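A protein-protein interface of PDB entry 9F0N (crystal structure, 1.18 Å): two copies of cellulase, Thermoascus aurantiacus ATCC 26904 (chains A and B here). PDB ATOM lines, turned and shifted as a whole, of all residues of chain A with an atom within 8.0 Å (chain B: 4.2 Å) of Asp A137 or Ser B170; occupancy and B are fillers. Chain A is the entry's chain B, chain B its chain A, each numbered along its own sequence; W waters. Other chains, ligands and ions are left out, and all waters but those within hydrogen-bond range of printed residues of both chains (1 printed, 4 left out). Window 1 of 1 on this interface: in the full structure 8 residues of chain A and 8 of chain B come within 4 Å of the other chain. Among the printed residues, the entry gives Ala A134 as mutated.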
ATOM      1  N   TYR A  96      35.890 -25.706  -7.144  1.00  0.00           N
ATOM      2  CA  TYR A  96      34.767 -26.063  -6.264  1.00  0.00           C
ATOM      3  C   TYR A  96      33.920 -24.851  -5.918  1.00  0.00           C
ATOM      4  O   TYR A  96      33.283 -24.816  -4.863  1.00  0.00           O
ATOM      5  CB  TYR A  96      35.251 -26.811  -5.001  1.00  0.00           C
ATOM      6  CG  TYR A  96      36.116 -28.011  -5.326  1.00  0.00           C
ATOM      7  CD1 TYR A  96      35.542 -29.223  -5.676  1.00  0.00           C
ATOM      8  CD2 TYR A  96      37.519 -27.925  -5.324  1.00  0.00           C
ATOM      9  CE1 TYR A  96      36.323 -30.319  -5.993  1.00  0.00           C
ATOM     10  CE2 TYR A  96      38.304 -29.023  -5.637  1.00  0.00           C
ATOM     11  CZ  TYR A  96      37.698 -30.205  -5.967  1.00  0.00           C
ATOM     12  OH  TYR A  96      38.483 -31.307  -6.277  1.00  0.00           O
ATOM     13  N   GLY A  97      33.895 -23.848  -6.797  1.00  0.00           N
ATOM     14  CA  GLY A  97      33.139 -22.643  -6.521  1.00  0.00           C
ATOM     15  C   GLY A  97      33.728 -21.762  -5.441  1.00  0.00           C
ATOM     16  O   GLY A  97      33.016 -20.896  -4.918  1.00  0.00           O
ATOM     17  N   ARG A  98      35.003 -21.954  -5.092  1.00  0.00           N
ATOM     18  CA  ARG A  98      35.633 -21.304  -3.954  1.00  0.00           C
ATOM     19  C   ARG A  98      36.986 -20.737  -4.366  1.00  0.00           C
ATOM     20  O   ARG A  98      37.654 -21.256  -5.263  1.00  0.00           O
ATOM     21  CB  ARG A  98      35.787 -22.300  -2.796  1.00  0.00           C
ATOM     22  CG  ARG A  98      34.472 -22.621  -2.090  1.00  0.00           C
ATOM     23  CD  ARG A  98      34.464 -24.018  -1.490  1.00  0.00           C
ATOM     24  NE  ARG A  98      33.273 -24.229  -0.656  1.00  0.00           N
ATOM     25  CZ  ARG A  98      32.063 -24.509  -1.115  1.00  0.00           C
ATOM     26  NH1 ARG A  98      31.832 -24.668  -2.410  1.00  0.00           N
ATOM     27  NH2 ARG A  98      31.049 -24.613  -0.252  1.00  0.00           N
ATOM     28  N   ILE A 103      33.485 -19.276  -0.605  1.00  0.00           N
ATOM     29  CA  ILE A 103      32.590 -19.300  -1.756  1.00  0.00           C
ATOM     30  C   ILE A 103      32.764 -18.030  -2.580  1.00  0.00           C
ATOM     31  O   ILE A 103      32.870 -16.922  -2.038  1.00  0.00           O
ATOM     32  CB  ILE A 103      31.139 -19.468  -1.273  1.00  0.00           C
ATOM     33  CG1 ILE A 103      30.922 -20.912  -0.813  1.00  0.00           C
ATOM     34  CG2 ILE A 103      30.125 -19.082  -2.372  1.00  0.00           C
ATOM     35  CD1 ILE A 103      29.632 -21.100  -0.005  1.00  0.00           C
ATOM     36  N   ALA A 134      33.034 -28.555 -10.151  1.00  0.00           N
ATOM     37  CA  ALA A 134      32.295 -29.162  -9.027  1.00  0.00           C
ATOM     38  C   ALA A 134      31.871 -28.176  -7.923  1.00  0.00           C
ATOM     39  O   ALA A 134      32.201 -28.338  -6.743  1.00  0.00           O
ATOM     40  CB  ALA A 134      33.076 -30.365  -8.477  1.00  0.00           C
ATOM     41  N   TYR A 135      31.069 -27.181  -8.304  1.00  0.00           N
ATOM     42  CA  TYR A 135      30.374 -26.354  -7.314  1.00  0.00           C
ATOM     43  C   TYR A 135      29.633 -27.264  -6.329  1.00  0.00           C
ATOM     44  O   TYR A 135      29.085 -28.303  -6.713  1.00  0.00           O
ATOM     45  CB  TYR A 135      29.333 -25.479  -8.016  1.00  0.00           C
ATOM     46  CG  TYR A 135      29.855 -24.550  -9.105  1.00  0.00           C
ATOM     47  CD1 TYR A 135      29.906 -24.962 -10.440  1.00  0.00           C
ATOM     48  CD2 TYR A 135      30.260 -23.253  -8.798  1.00  0.00           C
ATOM     49  CE1 TYR A 135      30.349 -24.125 -11.444  1.00  0.00           C
ATOM     50  CE2 TYR A 135      30.717 -22.399  -9.805  1.00  0.00           C
ATOM     51  CZ  TYR A 135      30.750 -22.843 -11.117  1.00  0.00           C
ATOM     52  OH  TYR A 135      31.217 -21.972 -12.091  1.00  0.00           O
ATOM     53  N   HIS A 136      29.592 -26.873  -5.056  1.00  0.00           N
ATOM     54  CA  HIS A 136      28.860 -27.669  -4.061  1.00  0.00           C
ATOM     55  C   HIS A 136      28.540 -26.803  -2.850  1.00  0.00           C
ATOM     56  O   HIS A 136      29.225 -25.812  -2.580  1.00  0.00           O
ATOM     57  CB  HIS A 136      29.670 -28.899  -3.635  1.00  0.00           C
ATOM     58  CG  HIS A 136      30.937 -28.558  -2.913  1.00  0.00           C
ATOM     59  ND1 HIS A 136      31.020 -28.491  -1.535  1.00  0.00           N
ATOM     60  CD2 HIS A 136      32.165 -28.227  -3.385  1.00  0.00           C
ATOM     61  CE1 HIS A 136      32.255 -28.165  -1.192  1.00  0.00           C
ATOM     62  NE2 HIS A 136      32.967 -27.996  -2.292  1.00  0.00           N
ATOM     63  N   ASP A 137      27.527 -27.221  -2.079  1.00  0.00           N
ATOM     64  CA  ASP A 137      27.189 -26.610  -0.782  1.00  0.00           C
ATOM     65  C   ASP A 137      27.162 -25.086  -0.857  1.00  0.00           C
ATOM     66  O   ASP A 137      27.832 -24.392  -0.101  1.00  0.00           O
ATOM     67  CB  ASP A 137      28.133 -27.105   0.321  1.00  0.00           C
ATOM     68  CG  ASP A 137      28.074 -28.592   0.473  1.00  0.00           C
ATOM     69  OD1 ASP A 137      27.017 -29.111   0.893  1.00  0.00           O
ATOM     70  OD2 ASP A 137      29.053 -29.270   0.130  1.00  0.00           O
ATOM     71  N   MET A 138      26.359 -24.574  -1.781  1.00  0.00           N
ATOM     72  CA  MET A 138      26.272 -23.137  -2.011  1.00  0.00           C
ATOM     73  C   MET A 138      24.931 -22.852  -2.678  1.00  0.00           C
ATOM     74  O   MET A 138      24.245 -23.750  -3.175  1.00  0.00           O
ATOM     75  CB  MET A 138      27.460 -22.610  -2.835  1.00  0.00           C
ATOM     76  CG  MET A 138      27.605 -23.281  -4.164  1.00  0.00           C
ATOM     77  SD  MET A 138      29.248 -23.028  -4.904  1.00  0.00           S
ATOM     78  CE  MET A 138      29.175 -21.302  -5.401  1.00  0.00           C
ATOM     79  N   ASP A 139      24.568 -21.577  -2.691  1.00  0.00           N
ATOM     80  CA  ASP A 139      23.258 -21.172  -3.174  1.00  0.00           C
ATOM     81  C   ASP A 139      23.084 -21.524  -4.655  1.00  0.00           C
ATOM     82  O   ASP A 139      23.978 -21.293  -5.473  1.00  0.00           O
ATOM     83  CB  ASP A 139      23.145 -19.661  -2.966  1.00  0.00           C
ATOM     84  CG  ASP A 139      21.831 -19.111  -3.438  1.00  0.00           C
ATOM     85  OD1 ASP A 139      20.875 -19.095  -2.634  1.00  0.00           O
ATOM     86  OD2 ASP A 139      21.743 -18.701  -4.604  1.00  0.00           O
ATOM     87  N   GLN A 140      21.908 -22.061  -5.011  1.00  0.00           N
ATOM     88  CA  GLN A 140      21.682 -22.585  -6.357  1.00  0.00           C
ATOM     89  C   GLN A 140      21.564 -21.477  -7.399  1.00  0.00           C
ATOM     90  O   GLN A 140      21.973 -21.666  -8.557  1.00  0.00           O
ATOM     91  CB  GLN A 140      20.413 -23.442  -6.344  1.00  0.00           C
ATOM     92  CG  GLN A 140      20.172 -24.157  -7.651  1.00  0.00           C
ATOM     93  CD  GLN A 140      21.283 -25.144  -7.994  1.00  0.00           C
ATOM     94  OE1 GLN A 140      21.862 -25.782  -7.108  1.00  0.00           O
ATOM     95  NE2 GLN A 140      21.604 -25.264  -9.266  1.00  0.00           N
ATOM     96  N   LEU A 142      23.177 -18.608  -7.098  1.00  0.00           N
ATOM     97  CA  LEU A 142      24.565 -18.191  -7.257  1.00  0.00           C
ATOM     98  C   LEU A 142      25.302 -19.082  -8.253  1.00  0.00           C
ATOM     99  O   LEU A 142      26.052 -18.577  -9.099  1.00  0.00           O
ATOM    100  CB  LEU A 142      25.264 -18.169  -5.898  1.00  0.00           C
ATOM    101  CG  LEU A 142      26.774 -17.871  -5.922  1.00  0.00           C
ATOM    102  CD1 LEU A 142      27.051 -16.460  -6.464  1.00  0.00           C
ATOM    103  CD2 LEU A 142      27.346 -18.027  -4.527  1.00  0.00           C
ATOM    104  N   VAL A 143      25.113 -20.409  -8.188  1.00  0.00           N
ATOM    105  CA  VAL A 143      25.798 -21.283  -9.153  1.00  0.00           C
ATOM    106  C   VAL A 143      25.402 -20.918 -10.581  1.00  0.00           C
ATOM    107  O   VAL A 143      26.243 -20.824 -11.479  1.00  0.00           O
ATOM    108  CB  VAL A 143      25.523 -22.767  -8.855  1.00  0.00           C
ATOM    109  CG1 VAL A 143      26.072 -23.646  -9.974  1.00  0.00           C
ATOM    110  CG2 VAL A 143      26.127 -23.155  -7.510  1.00  0.00           C
ATOM    111  N   GLY A 168      27.287 -27.794 -12.637  1.00  0.00           N
ATOM    112  CA  GLY A 168      26.267 -27.533 -11.653  1.00  0.00           C
ATOM    113  C   GLY A 168      26.714 -27.750 -10.218  1.00  0.00           C
ATOM    114  O   GLY A 168      27.856 -28.101  -9.919  1.00  0.00           O
ATOM    115  N   ASN A 169      25.752 -27.534  -9.321  1.00  0.00           N
ATOM    116  CA  ASN A 169      25.882 -27.778  -7.888  1.00  0.00           C
ATOM    117  C   ASN A 169      25.900 -29.290  -7.616  1.00  0.00           C
ATOM    118  O   ASN A 169      25.818 -30.118  -8.529  1.00  0.00           O
ATOM    119  CB  ASN A 169      24.706 -27.082  -7.202  1.00  0.00           C
ATOM    120  CG  ASN A 169      25.036 -26.525  -5.845  1.00  0.00           C
ATOM    121  OD1 ASN A 169      25.975 -26.961  -5.192  1.00  0.00           O
ATOM    122  ND2 ASN A 169      24.246 -25.566  -5.390  1.00  0.00           N
ATOM    123  N   SER A 170      25.996 -29.662  -6.337  1.00  0.00           N
ATOM    124  CA  SER A 170      26.092 -31.077  -5.947  1.00  0.00           C
ATOM    125  C   SER A 170      27.263 -31.748  -6.654  1.00  0.00           C
ATOM    126  O   SER A 170      27.168 -32.880  -7.134  1.00  0.00           O
ATOM    127  CB  SER A 170      24.770 -31.839  -6.174  1.00  0.00           C
ATOM    128  OG  SER A 170      23.818 -31.496  -5.176  1.00  0.00           O
ATOM    129  N   TRP A 171      28.388 -31.032  -6.717  1.00  0.00           N
ATOM    130  CA  TRP A 171      29.609 -31.566  -7.309  1.00  0.00           C
ATOM    131  C   TRP A 171      29.404 -31.949  -8.768  1.00  0.00           C
ATOM    132  O   TRP A 171      30.071 -32.863  -9.290  1.00  0.00           O
ATOM    133  CB  TRP A 171      30.204 -32.722  -6.491  1.00  0.00           C
ATOM    134  CG  TRP A 171      30.260 -32.486  -4.986  1.00  0.00           C
ATOM    135  CD1 TRP A 171      29.241 -32.642  -4.096  1.00  0.00           C
ATOM    136  CD2 TRP A 171      31.410 -32.086  -4.220  1.00  0.00           C
ATOM    137  NE1 TRP A 171      29.681 -32.358  -2.813  1.00  0.00           N
ATOM    138  CE2 TRP A 171      31.002 -32.014  -2.864  1.00  0.00           C
ATOM    139  CE3 TRP A 171      32.737 -31.798  -4.542  1.00  0.00           C
ATOM    140  CZ2 TRP A 171      31.886 -31.658  -1.831  1.00  0.00           C
ATOM    141  CZ3 TRP A 171      33.625 -31.447  -3.502  1.00  0.00           C
ATOM    142  CH2 TRP A 171      33.180 -31.379  -2.171  1.00  0.00           C
ATOM    143  N   TYR B 135      18.796 -34.469   4.914  1.00  0.00           N
ATOM    144  CA  TYR B 135      18.479 -34.134   3.527  1.00  0.00           C
ATOM    145  C   TYR B 135      19.756 -33.679   2.809  1.00  0.00           C
ATOM    146  O   TYR B 135      20.579 -32.952   3.373  1.00  0.00           O
ATOM    147  CB  TYR B 135      17.468 -32.980   3.481  1.00  0.00           C
ATOM    148  CG  TYR B 135      16.169 -33.230   4.205  1.00  0.00           C
ATOM    149  CD1 TYR B 135      15.994 -32.838   5.533  1.00  0.00           C
ATOM    150  CD2 TYR B 135      15.083 -33.803   3.538  1.00  0.00           C
ATOM    151  CE1 TYR B 135      14.780 -33.049   6.196  1.00  0.00           C
ATOM    152  CE2 TYR B 135      13.865 -34.003   4.189  1.00  0.00           C
ATOM    153  CZ  TYR B 135      13.715 -33.618   5.509  1.00  0.00           C
ATOM    154  OH  TYR B 135      12.492 -33.837   6.157  1.00  0.00           O
ATOM    155  N   ASN B 169      19.115 -29.021   4.267  1.00  0.00           N
ATOM    156  CA  ASN B 169      19.919 -29.554   3.169  1.00  0.00           C
ATOM    157  C   ASN B 169      21.421 -29.514   3.520  1.00  0.00           C
ATOM    158  O   ASN B 169      21.829 -29.123   4.616  1.00  0.00           O
ATOM    159  CB  ASN B 169      19.628 -28.717   1.919  1.00  0.00           C
ATOM    160  CG  ASN B 169      19.552 -29.537   0.643  1.00  0.00           C
ATOM    161  OD1 ASN B 169      20.200 -30.578   0.507  1.00  0.00           O
ATOM    162  ND2 ASN B 169      18.777 -29.055  -0.312  1.00  0.00           N
ATOM    163  N   SER B 170      22.254 -29.989   2.596  1.00  0.00           N
ATOM    164  CA  SER B 170      23.697 -30.134   2.865  1.00  0.00           C
ATOM    165  C   SER B 170      23.925 -31.011   4.089  1.00  0.00           C
ATOM    166  O   SER B 170      24.784 -30.728   4.938  1.00  0.00           O
ATOM    167  CB  SER B 170      24.451 -28.791   2.961  1.00  0.00           C
ATOM    168  OG  SER B 170      24.632 -28.203   1.665  1.00  0.00           O
ATOM    169  N   TRP B 171      23.165 -32.108   4.161  1.00  0.00           N
ATOM    170  CA  TRP B 171      23.325 -33.097   5.225  1.00  0.00           C
ATOM    171  C   TRP B 171      23.099 -32.456   6.590  1.00  0.00           C
ATOM    172  O   TRP B 171      23.672 -32.855   7.604  1.00  0.00           O
ATOM    173  CB  TRP B 171      24.678 -33.831   5.167  1.00  0.00           C
ATOM    174  CG  TRP B 171      25.064 -34.391   3.811  1.00  0.00           C
ATOM    175  CD1 TRP B 171      25.618 -33.697   2.771  1.00  0.00           C
ATOM    176  CD2 TRP B 171      24.910 -35.748   3.361  1.00  0.00           C
ATOM    177  NE1 TRP B 171      25.837 -34.546   1.703  1.00  0.00           N
ATOM    178  CE2 TRP B 171      25.410 -35.805   2.039  1.00  0.00           C
ATOM    179  CE3 TRP B 171      24.429 -36.913   3.953  1.00  0.00           C
ATOM    180  CZ2 TRP B 171      25.431 -36.993   1.297  1.00  0.00           C
ATOM    181  CZ3 TRP B 171      24.455 -38.096   3.220  1.00  0.00           C
ATOM    182  CH2 TRP B 171      24.940 -38.121   1.901  1.00  0.00           C
ATOM    183  N   THR B 172      22.248 -31.436   6.594  1.00  0.00           N
ATOM    184  CA  THR B 172      21.937 -30.606   7.759  1.00  0.00           C
ATOM    185  C   THR B 172      23.182 -30.089   8.500  1.00  0.00           C
ATOM    186  O   THR B 172      23.151 -29.817   9.709  1.00  0.00           O
ATOM    187  CB  THR B 172      20.829 -31.202   8.662  1.00  0.00           C
ATOM    188  OG1 THR B 172      20.116 -30.138   9.304  1.00  0.00           O
ATOM    189  CG2 THR B 172      21.322 -32.235   9.676  1.00  0.00           C
ATOM    190  N   GLY B 173      24.280 -29.866   7.772  1.00  0.00           N
ATOM    191  CA  GLY B 173      25.513 -29.449   8.437  1.00  0.00           C
ATOM    192  C   GLY B 173      25.399 -28.056   9.024  1.00  0.00           C
ATOM    193  O   GLY B 173      24.816 -27.153   8.424  1.00  0.00           O
ATOM    194  N   THR B 176      27.618 -25.425   6.900  1.00  0.00           N
ATOM    195  CA  THR B 176      27.101 -25.063   5.589  1.00  0.00           C
ATOM    196  C   THR B 176      25.722 -24.416   5.677  1.00  0.00           C
ATOM    197  O   THR B 176      25.171 -24.016   4.647  1.00  0.00           O
ATOM    198  CB  THR B 176      27.004 -26.329   4.724  1.00  0.00           C
ATOM    199  OG1 THR B 176      26.357 -27.361   5.475  1.00  0.00           O
ATOM    200  CG2 THR B 176      28.381 -26.846   4.335  1.00  0.00           C
ATOM    201  N   ASN B 179      24.879 -20.995   4.110  1.00  0.00           N
ATOM    202  CA  ASN B 179      25.102 -20.935   2.676  1.00  0.00           C
ATOM    203  C   ASN B 179      23.938 -21.496   1.871  1.00  0.00           C
ATOM    204  O   ASN B 179      23.756 -21.092   0.717  1.00  0.00           O
ATOM    205  CB  ASN B 179      26.403 -21.660   2.344  1.00  0.00           C
ATOM    206  CG  ASN B 179      27.643 -20.930   2.902  1.00  0.00           C
ATOM    207  OD1 ASN B 179      27.673 -19.696   2.978  1.00  0.00           O
ATOM    208  ND2 ASN B 179      28.652 -21.696   3.295  1.00  0.00           N
ATOM    209  N   VAL B 180      23.134 -22.407   2.449  1.00  0.00           N
ATOM    210  CA  VAL B 180      22.078 -23.058   1.669  1.00  0.00           C
ATOM    211  C   VAL B 180      20.682 -23.044   2.280  1.00  0.00           C
ATOM    212  O   VAL B 180      19.699 -23.135   1.542  1.00  0.00           O
ATOM    213  CB  VAL B 180      22.446 -24.494   1.248  1.00  0.00           C
ATOM    214  CG1 VAL B 180      23.774 -24.543   0.469  1.00  0.00           C
ATOM    215  CG2 VAL B 180      22.453 -25.429   2.445  1.00  0.00           C
HETATM  216  O   HOH W   1      25.916 -19.916  -0.869  1.00  0.00           O
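Printed residues of chain B that touch a printed residue of chain A: Ser B170, Asn B179 and Val B180. Hydrophobic or aromatic side chains of chain B that line the printed part of chain A: Val B180. Among the printed residues, 6 pairs touch across the chains.
ND2 of Asn B179 touches CD1 of Ile A103 (3.5 Å). Asn B179 touches Asp A137. Val B180 touches Asp A137 (CG1 to C, 3.7 Å). Val B180 touches Met A138. O of Asn B179 touches N of Asp A139, at 3.5 Å.
OG of Ser B170 is in hydrogen-bond range of OD1 of Asp A137, at 2.7 Å.
O of Met A138 sits at hydrogen-bond distance from ND2 of Asn A169, 2.9 Å away. ND1 of His A136 is in hydrogen-bond range of OD2 of Asp A137, at 2.7 Å. The backbone NH (N) of Leu A142 is in hydrogen-bond range of the side-chain carboxylate (OD2) of Asp A139 (2.9 Å). O of Asp A137 is in hydrogen-bond range of NH2 of Arg A98. The backbone NH (N) of Asp A137 sits at hydrogen-bond distance from the side-chain amide oxygen (OD1) of Asn A169 (3.5 Å). The backbone NH (N) of Ser B170 is in hydrogen-bond range of the backbone carbonyl oxygen (O) of Tyr B135, 3.5 Å away.
Water W1 bridges the backbone NH of Asp A139 (2.8 Å) and the backbone carbonyl oxygen of Asn B179 (2.9 Å).
Ser B170 touches just one residue of chain A: Asp A137. Printed residues of chain A within 4 Å of Val B180: Asp A137 (3.7 Å) and Met A138 (3.4 Å). Printed residues of chain A within 4 Å of Asn B179: Ile A103 (3.5 Å), Asp A137 (3.9 Å) and Asp A139 (3.5 Å). The nearest residue of chain B that does not touch Asp A137 is Thr B176 (4.03 Å). The nearest residue of chain A that does not touch Ser B170 is Met A138 (5.3 Å). The nearest printed residue of chain A that does not touch Asn B179 is Met A138 (4.001 Å).
Positions printed for both chains: 135, 169, 170 and 171. Of the 6 pairs that touch across the chains among the printed residues, none has its exchanged pair printed and touching as well.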
